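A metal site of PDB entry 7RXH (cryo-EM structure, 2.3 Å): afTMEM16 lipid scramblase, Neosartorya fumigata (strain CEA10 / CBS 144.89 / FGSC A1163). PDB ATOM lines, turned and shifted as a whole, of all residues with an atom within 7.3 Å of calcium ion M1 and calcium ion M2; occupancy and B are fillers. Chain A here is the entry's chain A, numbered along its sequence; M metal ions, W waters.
The side-chain amino group (NZ) of Lys 550 lies close to the side-chain carboxylate (OE2) of Glu 445 (2.6 Å).
The side-chain carboxylate (OD2) of Asp 511 lies within salt-bridge range of the side-chain amino group (NZ) of Lys 550 (3.4 Å).
The side-chain amino group (NZ) of Lys 550 sits close to the side-chain carboxylate (OD1) of Asp 547.
ND2 of Asn 539 lies close to OE2 of Glu 543, at 3.2 Å.
OD2 of Asp 511 lies within hydrogen-bond range of OH of Tyr 506.
Lys 550 touches calcium ion M1 (NZ to CA, 3.9 Å).
Of the 25 residues printed, 6 come within 4 Å of calcium ion M1.
Three residues have an atom within 4 Å of calcium ion M2: Glu 445, Glu 514 and Glu 543.
Calcium ion M1 is bound by OE1 of Glu 543 (2.4 Å), OE2 of Glu 445 (2.4 Å), OD1 of Asp 511 (2.6 Å), water W1 (2.6 Å), OE1 of Glu 514 (2.6 Å), OD1 of Asp 547 (2.7 Å) and OD2 of Asp 547 (2.7 Å).
Calcium ion M2 is bound by the side-chain carboxylate (OE2) of Glu 514 (2.4 Å), water W2 (2.5 Å), the side-chain carboxylate (OE1) of Glu 445 (2.6 Å), the side-chain carboxylate (OE2) of Glu 543 (2.7 Å) and the side-chain carboxylate (OE1) of Glu 543 (2.7 Å).
Calcium ion M2 has five donor atoms within binding distance.
Water W1 lies within hydrogen-bond range of OH of Tyr 180 and O of Asp 511.
Water W2 bridges the side-chain amide oxygen (OD1) of Asn 539 and the backbone carbonyl oxygen (O) of Gln 438.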
ATOM      1  N   TYR A 180      13.986 -38.004  -8.534  1.00  0.00           N
ATOM      2  CA  TYR A 180      14.175 -37.281  -7.286  1.00  0.00           C
ATOM      3  C   TYR A 180      13.198 -37.742  -6.227  1.00  0.00           C
ATOM      4  O   TYR A 180      13.582 -37.982  -5.076  1.00  0.00           O
ATOM      5  CB  TYR A 180      14.050 -35.778  -7.482  1.00  0.00           C
ATOM      6  CG  TYR A 180      13.816 -35.067  -6.156  1.00  0.00           C
ATOM      7  CD1 TYR A 180      14.805 -35.034  -5.183  1.00  0.00           C
ATOM      8  CD2 TYR A 180      12.604 -34.457  -5.875  1.00  0.00           C
ATOM      9  CE1 TYR A 180      14.595 -34.404  -3.984  1.00  0.00           C
ATOM     10  CE2 TYR A 180      12.394 -33.826  -4.677  1.00  0.00           C
ATOM     11  CZ  TYR A 180      13.392 -33.804  -3.730  1.00  0.00           C
ATOM     12  OH  TYR A 180      13.182 -33.174  -2.531  1.00  0.00           O
ATOM     13  N   LEU A 184      14.028 -39.609  -2.733  1.00  0.00           N
ATOM     14  CA  LEU A 184      13.604 -39.050  -1.452  1.00  0.00           C
ATOM     15  C   LEU A 184      12.785 -40.051  -0.657  1.00  0.00           C
ATOM     16  O   LEU A 184      12.961 -40.193   0.553  1.00  0.00           O
ATOM     17  CB  LEU A 184      12.811 -37.768  -1.671  1.00  0.00           C
ATOM     18  CG  LEU A 184      12.375 -37.005  -0.425  1.00  0.00           C
ATOM     19  CD1 LEU A 184      13.538 -36.782   0.516  1.00  0.00           C
ATOM     20  CD2 LEU A 184      11.735 -35.689  -0.785  1.00  0.00           C
ATOM     21  N   ALA A 437      18.091 -25.164  10.942  1.00  0.00           N
ATOM     22  CA  ALA A 437      18.288 -24.935   9.525  1.00  0.00           C
ATOM     23  C   ALA A 437      17.241 -25.649   8.683  1.00  0.00           C
ATOM     24  O   ALA A 437      16.784 -25.109   7.681  1.00  0.00           O
ATOM     25  CB  ALA A 437      19.692 -25.361   9.102  1.00  0.00           C
ATOM     26  N   GLN A 438      16.812 -26.852   9.104  1.00  0.00           N
ATOM     27  CA  GLN A 438      15.767 -27.552   8.369  1.00  0.00           C
ATOM     28  C   GLN A 438      14.455 -26.782   8.400  1.00  0.00           C
ATOM     29  O   GLN A 438      13.796 -26.607   7.371  1.00  0.00           O
ATOM     30  CB  GLN A 438      15.557 -28.952   8.947  1.00  0.00           C
ATOM     31  CG  GLN A 438      16.824 -29.754   9.133  1.00  0.00           C
ATOM     32  CD  GLN A 438      17.489 -30.122   7.825  1.00  0.00           C
ATOM     33  OE1 GLN A 438      18.599 -29.687   7.537  1.00  0.00           O
ATOM     34  NE2 GLN A 438      16.808 -30.933   7.030  1.00  0.00           N
ATOM     35  N   ILE A 439      14.056 -26.299   9.590  1.00  0.00           N
ATOM     36  CA  ILE A 439      12.803 -25.563   9.705  1.00  0.00           C
ATOM     37  C   ILE A 439      12.879 -24.239   8.943  1.00  0.00           C
ATOM     38  O   ILE A 439      11.946 -23.878   8.200  1.00  0.00           O
ATOM     39  CB  ILE A 439      12.442 -25.341  11.182  1.00  0.00           C
ATOM     40  CG1 ILE A 439      12.262 -26.684  11.884  1.00  0.00           C
ATOM     41  CG2 ILE A 439      11.191 -24.507  11.313  1.00  0.00           C
ATOM     42  CD1 ILE A 439      12.325 -26.608  13.385  1.00  0.00           C
ATOM     43  N   VAL A 440      13.979 -23.503   9.088  1.00  0.00           N
ATOM     44  CA  VAL A 440      14.114 -22.214   8.410  1.00  0.00           C
ATOM     45  C   VAL A 440      14.192 -22.415   6.905  1.00  0.00           C
ATOM     46  O   VAL A 440      13.712 -21.581   6.134  1.00  0.00           O
ATOM     47  CB  VAL A 440      15.337 -21.466   8.958  1.00  0.00           C
ATOM     48  CG1 VAL A 440      15.597 -20.216   8.145  1.00  0.00           C
ATOM     49  CG2 VAL A 440      15.143 -21.129  10.421  1.00  0.00           C
ATOM     50  N   GLY A 441      14.801 -23.506   6.456  1.00  0.00           N
ATOM     51  CA  GLY A 441      14.864 -23.786   5.038  1.00  0.00           C
ATOM     52  C   GLY A 441      13.529 -24.181   4.473  1.00  0.00           C
ATOM     53  O   GLY A 441      13.191 -23.806   3.358  1.00  0.00           O
ATOM     54  N   PHE A 442      12.743 -24.954   5.231  1.00  0.00           N
ATOM     55  CA  PHE A 442      11.364 -25.206   4.837  1.00  0.00           C
ATOM     56  C   PHE A 442      10.603 -23.908   4.666  1.00  0.00           C
ATOM     57  O   PHE A 442       9.888 -23.716   3.669  1.00  0.00           O
ATOM     58  CB  PHE A 442      10.677 -26.105   5.871  1.00  0.00           C
ATOM     59  CG  PHE A 442       9.175 -26.122   5.758  1.00  0.00           C
ATOM     60  CD1 PHE A 442       8.554 -26.909   4.814  1.00  0.00           C
ATOM     61  CD2 PHE A 442       8.398 -25.357   6.607  1.00  0.00           C
ATOM     62  CE1 PHE A 442       7.175 -26.938   4.708  1.00  0.00           C
ATOM     63  CE2 PHE A 442       7.021 -25.374   6.508  1.00  0.00           C
ATOM     64  CZ  PHE A 442       6.411 -26.169   5.559  1.00  0.00           C
ATOM     65  N   ALA A 443      10.753 -22.987   5.622  1.00  0.00           N
ATOM     66  CA  ALA A 443      10.104 -21.688   5.513  1.00  0.00           C
ATOM     67  C   ALA A 443      10.540 -20.950   4.251  1.00  0.00           C
ATOM     68  O   ALA A 443       9.721 -20.662   3.367  1.00  0.00           O
ATOM     69  CB  ALA A 443      10.390 -20.848   6.756  1.00  0.00           C
ATOM     70  N   GLU A 445      11.859 -21.963   1.633  1.00  0.00           N
ATOM     71  CA  GLU A 445      11.685 -22.712   0.397  1.00  0.00           C
ATOM     72  C   GLU A 445      10.240 -22.770  -0.056  1.00  0.00           C
ATOM     73  O   GLU A 445       9.964 -22.627  -1.248  1.00  0.00           O
ATOM     74  CB  GLU A 445      12.229 -24.133   0.581  1.00  0.00           C
ATOM     75  CG  GLU A 445      12.232 -24.974  -0.669  1.00  0.00           C
ATOM     76  CD  GLU A 445      12.888 -26.321  -0.448  1.00  0.00           C
ATOM     77  OE1 GLU A 445      13.191 -26.660   0.716  1.00  0.00           O
ATOM     78  OE2 GLU A 445      13.112 -27.039  -1.439  1.00  0.00           O
ATOM     79  N   THR A 446       9.304 -22.981   0.866  1.00  0.00           N
ATOM     80  CA  THR A 446       7.889 -23.073   0.492  1.00  0.00           C
ATOM     81  C   THR A 446       7.087 -21.844   0.850  1.00  0.00           C
ATOM     82  O   THR A 446       6.316 -21.366   0.020  1.00  0.00           O
ATOM     83  CB  THR A 446       7.245 -24.298   1.143  1.00  0.00           C
ATOM     84  OG1 THR A 446       7.281 -24.175   2.572  1.00  0.00           O
ATOM     85  CG2 THR A 446       7.959 -25.574   0.723  1.00  0.00           C
ATOM     86  N   TYR A 506      11.321 -24.571 -11.968  1.00  0.00           N
ATOM     87  CA  TYR A 506      11.759 -25.613 -11.048  1.00  0.00           C
ATOM     88  C   TYR A 506      13.019 -26.299 -11.574  1.00  0.00           C
ATOM     89  O   TYR A 506      13.076 -26.699 -12.734  1.00  0.00           O
ATOM     90  CB  TYR A 506      10.661 -26.645 -10.831  1.00  0.00           C
ATOM     91  CG  TYR A 506      11.070 -27.759  -9.904  1.00  0.00           C
ATOM     92  CD1 TYR A 506      11.255 -27.532  -8.549  1.00  0.00           C
ATOM     93  CD2 TYR A 506      11.298 -29.042 -10.393  1.00  0.00           C
ATOM     94  CE1 TYR A 506      11.642 -28.547  -7.704  1.00  0.00           C
ATOM     95  CE2 TYR A 506      11.685 -30.057  -9.548  1.00  0.00           C
ATOM     96  CZ  TYR A 506      11.855 -29.805  -8.204  1.00  0.00           C
ATOM     97  OH  TYR A 506      12.243 -30.819  -7.359  1.00  0.00           O
ATOM     98  N   ASP A 510      18.282 -28.515  -7.327  1.00  0.00           N
ATOM     99  CA  ASP A 510      18.300 -27.842  -6.034  1.00  0.00           C
ATOM    100  C   ASP A 510      17.806 -28.764  -4.921  1.00  0.00           C
ATOM    101  O   ASP A 510      18.411 -28.824  -3.844  1.00  0.00           O
ATOM    102  CB  ASP A 510      17.450 -26.580  -6.081  1.00  0.00           C
ATOM    103  CG  ASP A 510      17.860 -25.654  -7.201  1.00  0.00           C
ATOM    104  OD1 ASP A 510      19.064 -25.559  -7.488  1.00  0.00           O
ATOM    105  OD2 ASP A 510      16.957 -25.024  -7.803  1.00  0.00           O
ATOM    106  N   ASP A 511      16.731 -29.504  -5.170  1.00  0.00           N
ATOM    107  CA  ASP A 511      16.202 -30.408  -4.166  1.00  0.00           C
ATOM    108  C   ASP A 511      17.149 -31.574  -3.927  1.00  0.00           C
ATOM    109  O   ASP A 511      17.345 -32.013  -2.783  1.00  0.00           O
ATOM    110  CB  ASP A 511      14.824 -30.895  -4.583  1.00  0.00           C
ATOM    111  CG  ASP A 511      13.757 -29.826  -4.405  1.00  0.00           C
ATOM    112  OD1 ASP A 511      14.010 -28.865  -3.670  1.00  0.00           O
ATOM    113  OD2 ASP A 511      12.676 -29.952  -5.007  1.00  0.00           O
ATOM    114  N   LEU A 512      17.751 -32.104  -5.000  1.00  0.00           N
ATOM    115  CA  LEU A 512      18.752 -33.155  -4.838  1.00  0.00           C
ATOM    116  C   LEU A 512      19.946 -32.652  -4.037  1.00  0.00           C
ATOM    117  O   LEU A 512      20.469 -33.366  -3.172  1.00  0.00           O
ATOM    118  CB  LEU A 512      19.193 -33.685  -6.190  1.00  0.00           C
ATOM    119  CG  LEU A 512      18.202 -34.637  -6.865  1.00  0.00           C
ATOM    120  CD1 LEU A 512      18.484 -34.715  -8.350  1.00  0.00           C
ATOM    121  CD2 LEU A 512      18.257 -36.004  -6.214  1.00  0.00           C
ATOM    122  N   GLU A 514      19.928 -30.281  -1.772  1.00  0.00           N
ATOM    123  CA  GLU A 514      19.516 -30.160  -0.377  1.00  0.00           C
ATOM    124  C   GLU A 514      19.518 -31.507   0.328  1.00  0.00           C
ATOM    125  O   GLU A 514      20.046 -31.641   1.433  1.00  0.00           O
ATOM    126  CB  GLU A 514      18.138 -29.509  -0.286  1.00  0.00           C
ATOM    127  CG  GLU A 514      17.616 -29.380   1.119  1.00  0.00           C
ATOM    128  CD  GLU A 514      16.164 -28.968   1.190  1.00  0.00           C
ATOM    129  OE1 GLU A 514      15.631 -28.465   0.178  1.00  0.00           O
ATOM    130  OE2 GLU A 514      15.551 -29.151   2.260  1.00  0.00           O
ATOM    131  N   MET A 515      18.964 -32.534  -0.318  1.00  0.00           N
ATOM    132  CA  MET A 515      18.922 -33.852   0.306  1.00  0.00           C
ATOM    133  C   MET A 515      20.314 -34.436   0.472  1.00  0.00           C
ATOM    134  O   MET A 515      20.605 -35.092   1.488  1.00  0.00           O
ATOM    135  CB  MET A 515      18.030 -34.795  -0.489  1.00  0.00           C
ATOM    136  CG  MET A 515      16.546 -34.517  -0.300  1.00  0.00           C
ATOM    137  SD  MET A 515      16.015 -34.567   1.423  1.00  0.00           S
ATOM    138  CE  MET A 515      15.958 -32.816   1.813  1.00  0.00           C
ATOM    139  N   GLN A 518      22.042 -32.723   3.377  1.00  0.00           N
ATOM    140  CA  GLN A 518      21.487 -33.260   4.615  1.00  0.00           C
ATOM    141  C   GLN A 518      22.088 -34.624   4.942  1.00  0.00           C
ATOM    142  O   GLN A 518      22.479 -34.904   6.089  1.00  0.00           O
ATOM    143  CB  GLN A 518      19.963 -33.360   4.481  1.00  0.00           C
ATOM    144  CG  GLN A 518      19.253 -33.742   5.747  1.00  0.00           C
ATOM    145  CD  GLN A 518      17.916 -34.369   5.475  1.00  0.00           C
ATOM    146  OE1 GLN A 518      17.824 -35.546   5.169  1.00  0.00           O
ATOM    147  NE2 GLN A 518      16.865 -33.578   5.585  1.00  0.00           N
ATOM    148  N   ASN A 539      11.726 -34.407   8.826  1.00  0.00           N
ATOM    149  CA  ASN A 539      11.859 -33.393   7.790  1.00  0.00           C
ATOM    150  C   ASN A 539      11.650 -33.980   6.409  1.00  0.00           C
ATOM    151  O   ASN A 539      11.105 -33.306   5.535  1.00  0.00           O
ATOM    152  CB  ASN A 539      13.227 -32.726   7.864  1.00  0.00           C
ATOM    153  CG  ASN A 539      13.439 -31.728   6.742  1.00  0.00           C
ATOM    154  OD1 ASN A 539      13.049 -30.573   6.844  1.00  0.00           O
ATOM    155  ND2 ASN A 539      14.053 -32.180   5.659  1.00  0.00           N
ATOM    156  N   VAL A 542       8.043 -34.604   5.610  1.00  0.00           N
ATOM    157  CA  VAL A 542       7.444 -33.330   5.224  1.00  0.00           C
ATOM    158  C   VAL A 542       8.002 -32.847   3.890  1.00  0.00           C
ATOM    159  O   VAL A 542       7.314 -32.142   3.141  1.00  0.00           O
ATOM    160  CB  VAL A 542       7.649 -32.288   6.340  1.00  0.00           C
ATOM    161  CG1 VAL A 542       7.351 -30.902   5.812  1.00  0.00           C
ATOM    162  CG2 VAL A 542       6.777 -32.606   7.532  1.00  0.00           C
ATOM    163  N   GLU A 543       9.235 -33.234   3.557  1.00  0.00           N
ATOM    164  CA  GLU A 543       9.915 -32.713   2.378  1.00  0.00           C
ATOM    165  C   GLU A 543       9.300 -33.241   1.103  1.00  0.00           C
ATOM    166  O   GLU A 543       9.173 -32.506   0.125  1.00  0.00           O
ATOM    167  CB  GLU A 543      11.397 -33.079   2.446  1.00  0.00           C
ATOM    168  CG  GLU A 543      12.263 -32.375   1.418  1.00  0.00           C
ATOM    169  CD  GLU A 543      12.630 -30.977   1.851  1.00  0.00           C
ATOM    170  OE1 GLU A 543      12.781 -30.108   0.978  1.00  0.00           O
ATOM    171  OE2 GLU A 543      12.761 -30.752   3.068  1.00  0.00           O
ATOM    172  N   LEU A 544       8.929 -34.528   1.086  1.00  0.00           N
ATOM    173  CA  LEU A 544       8.198 -35.079  -0.063  1.00  0.00           C
ATOM    174  C   LEU A 544       6.976 -34.235  -0.395  1.00  0.00           C
ATOM    175  O   LEU A 544       6.841 -33.721  -1.519  1.00  0.00           O
ATOM    176  CB  LEU A 544       7.789 -36.523   0.225  1.00  0.00           C
ATOM    177  CG  LEU A 544       8.886 -37.574   0.209  1.00  0.00           C
ATOM    178  CD1 LEU A 544       8.399 -38.868   0.827  1.00  0.00           C
ATOM    179  CD2 LEU A 544       9.327 -37.836  -1.209  1.00  0.00           C
ATOM    180  N   SER A 546       6.011 -31.204   0.734  1.00  0.00           N
ATOM    181  CA  SER A 546       6.234 -29.780   0.516  1.00  0.00           C
ATOM    182  C   SER A 546       6.948 -29.518  -0.799  1.00  0.00           C
ATOM    183  O   SER A 546       6.675 -28.507  -1.445  1.00  0.00           O
ATOM    184  CB  SER A 546       7.007 -29.182   1.685  1.00  0.00           C
ATOM    185  OG  SER A 546       8.399 -29.338   1.531  1.00  0.00           O
ATOM    186  N   ASP A 547       7.817 -30.419  -1.251  1.00  0.00           N
ATOM    187  CA  ASP A 547       8.437 -30.261  -2.555  1.00  0.00           C
ATOM    188  C   ASP A 547       7.439 -30.492  -3.669  1.00  0.00           C
ATOM    189  O   ASP A 547       7.453 -29.779  -4.686  1.00  0.00           O
ATOM    190  CB  ASP A 547       9.631 -31.210  -2.697  1.00  0.00           C
ATOM    191  CG  ASP A 547      10.895 -30.644  -2.103  1.00  0.00           C
ATOM    192  OD1 ASP A 547      10.947 -29.426  -1.871  1.00  0.00           O
ATOM    193  OD2 ASP A 547      11.844 -31.419  -1.873  1.00  0.00           O
ATOM    194  N   LYS A 550       5.482 -27.337  -3.803  1.00  0.00           N
ATOM    195  CA  LYS A 550       6.254 -26.291  -4.443  1.00  0.00           C
ATOM    196  C   LYS A 550       6.266 -26.450  -5.956  1.00  0.00           C
ATOM    197  O   LYS A 550       6.137 -25.466  -6.690  1.00  0.00           O
ATOM    198  CB  LYS A 550       7.682 -26.291  -3.896  1.00  0.00           C
ATOM    199  CG  LYS A 550       8.626 -25.343  -4.595  1.00  0.00           C
ATOM    200  CD  LYS A 550      10.007 -25.427  -4.000  1.00  0.00           C
ATOM    201  CE  LYS A 550      10.664 -26.762  -4.312  1.00  0.00           C
ATOM    202  NZ  LYS A 550      12.031 -26.846  -3.770  1.00  0.00           N
HETATM  203 CA    CA M   1      13.553 -29.384  -1.174  1.00  0.00          CA
HETATM  204 CA    CA M   2      13.412 -28.183   2.763  1.00  0.00          CA
HETATM  205  O   HOH W   1      14.990 -31.572  -1.000  1.00  0.00           O
HETATM  206  O   HOH W   2      13.668 -28.673   5.229  1.00  0.00           O
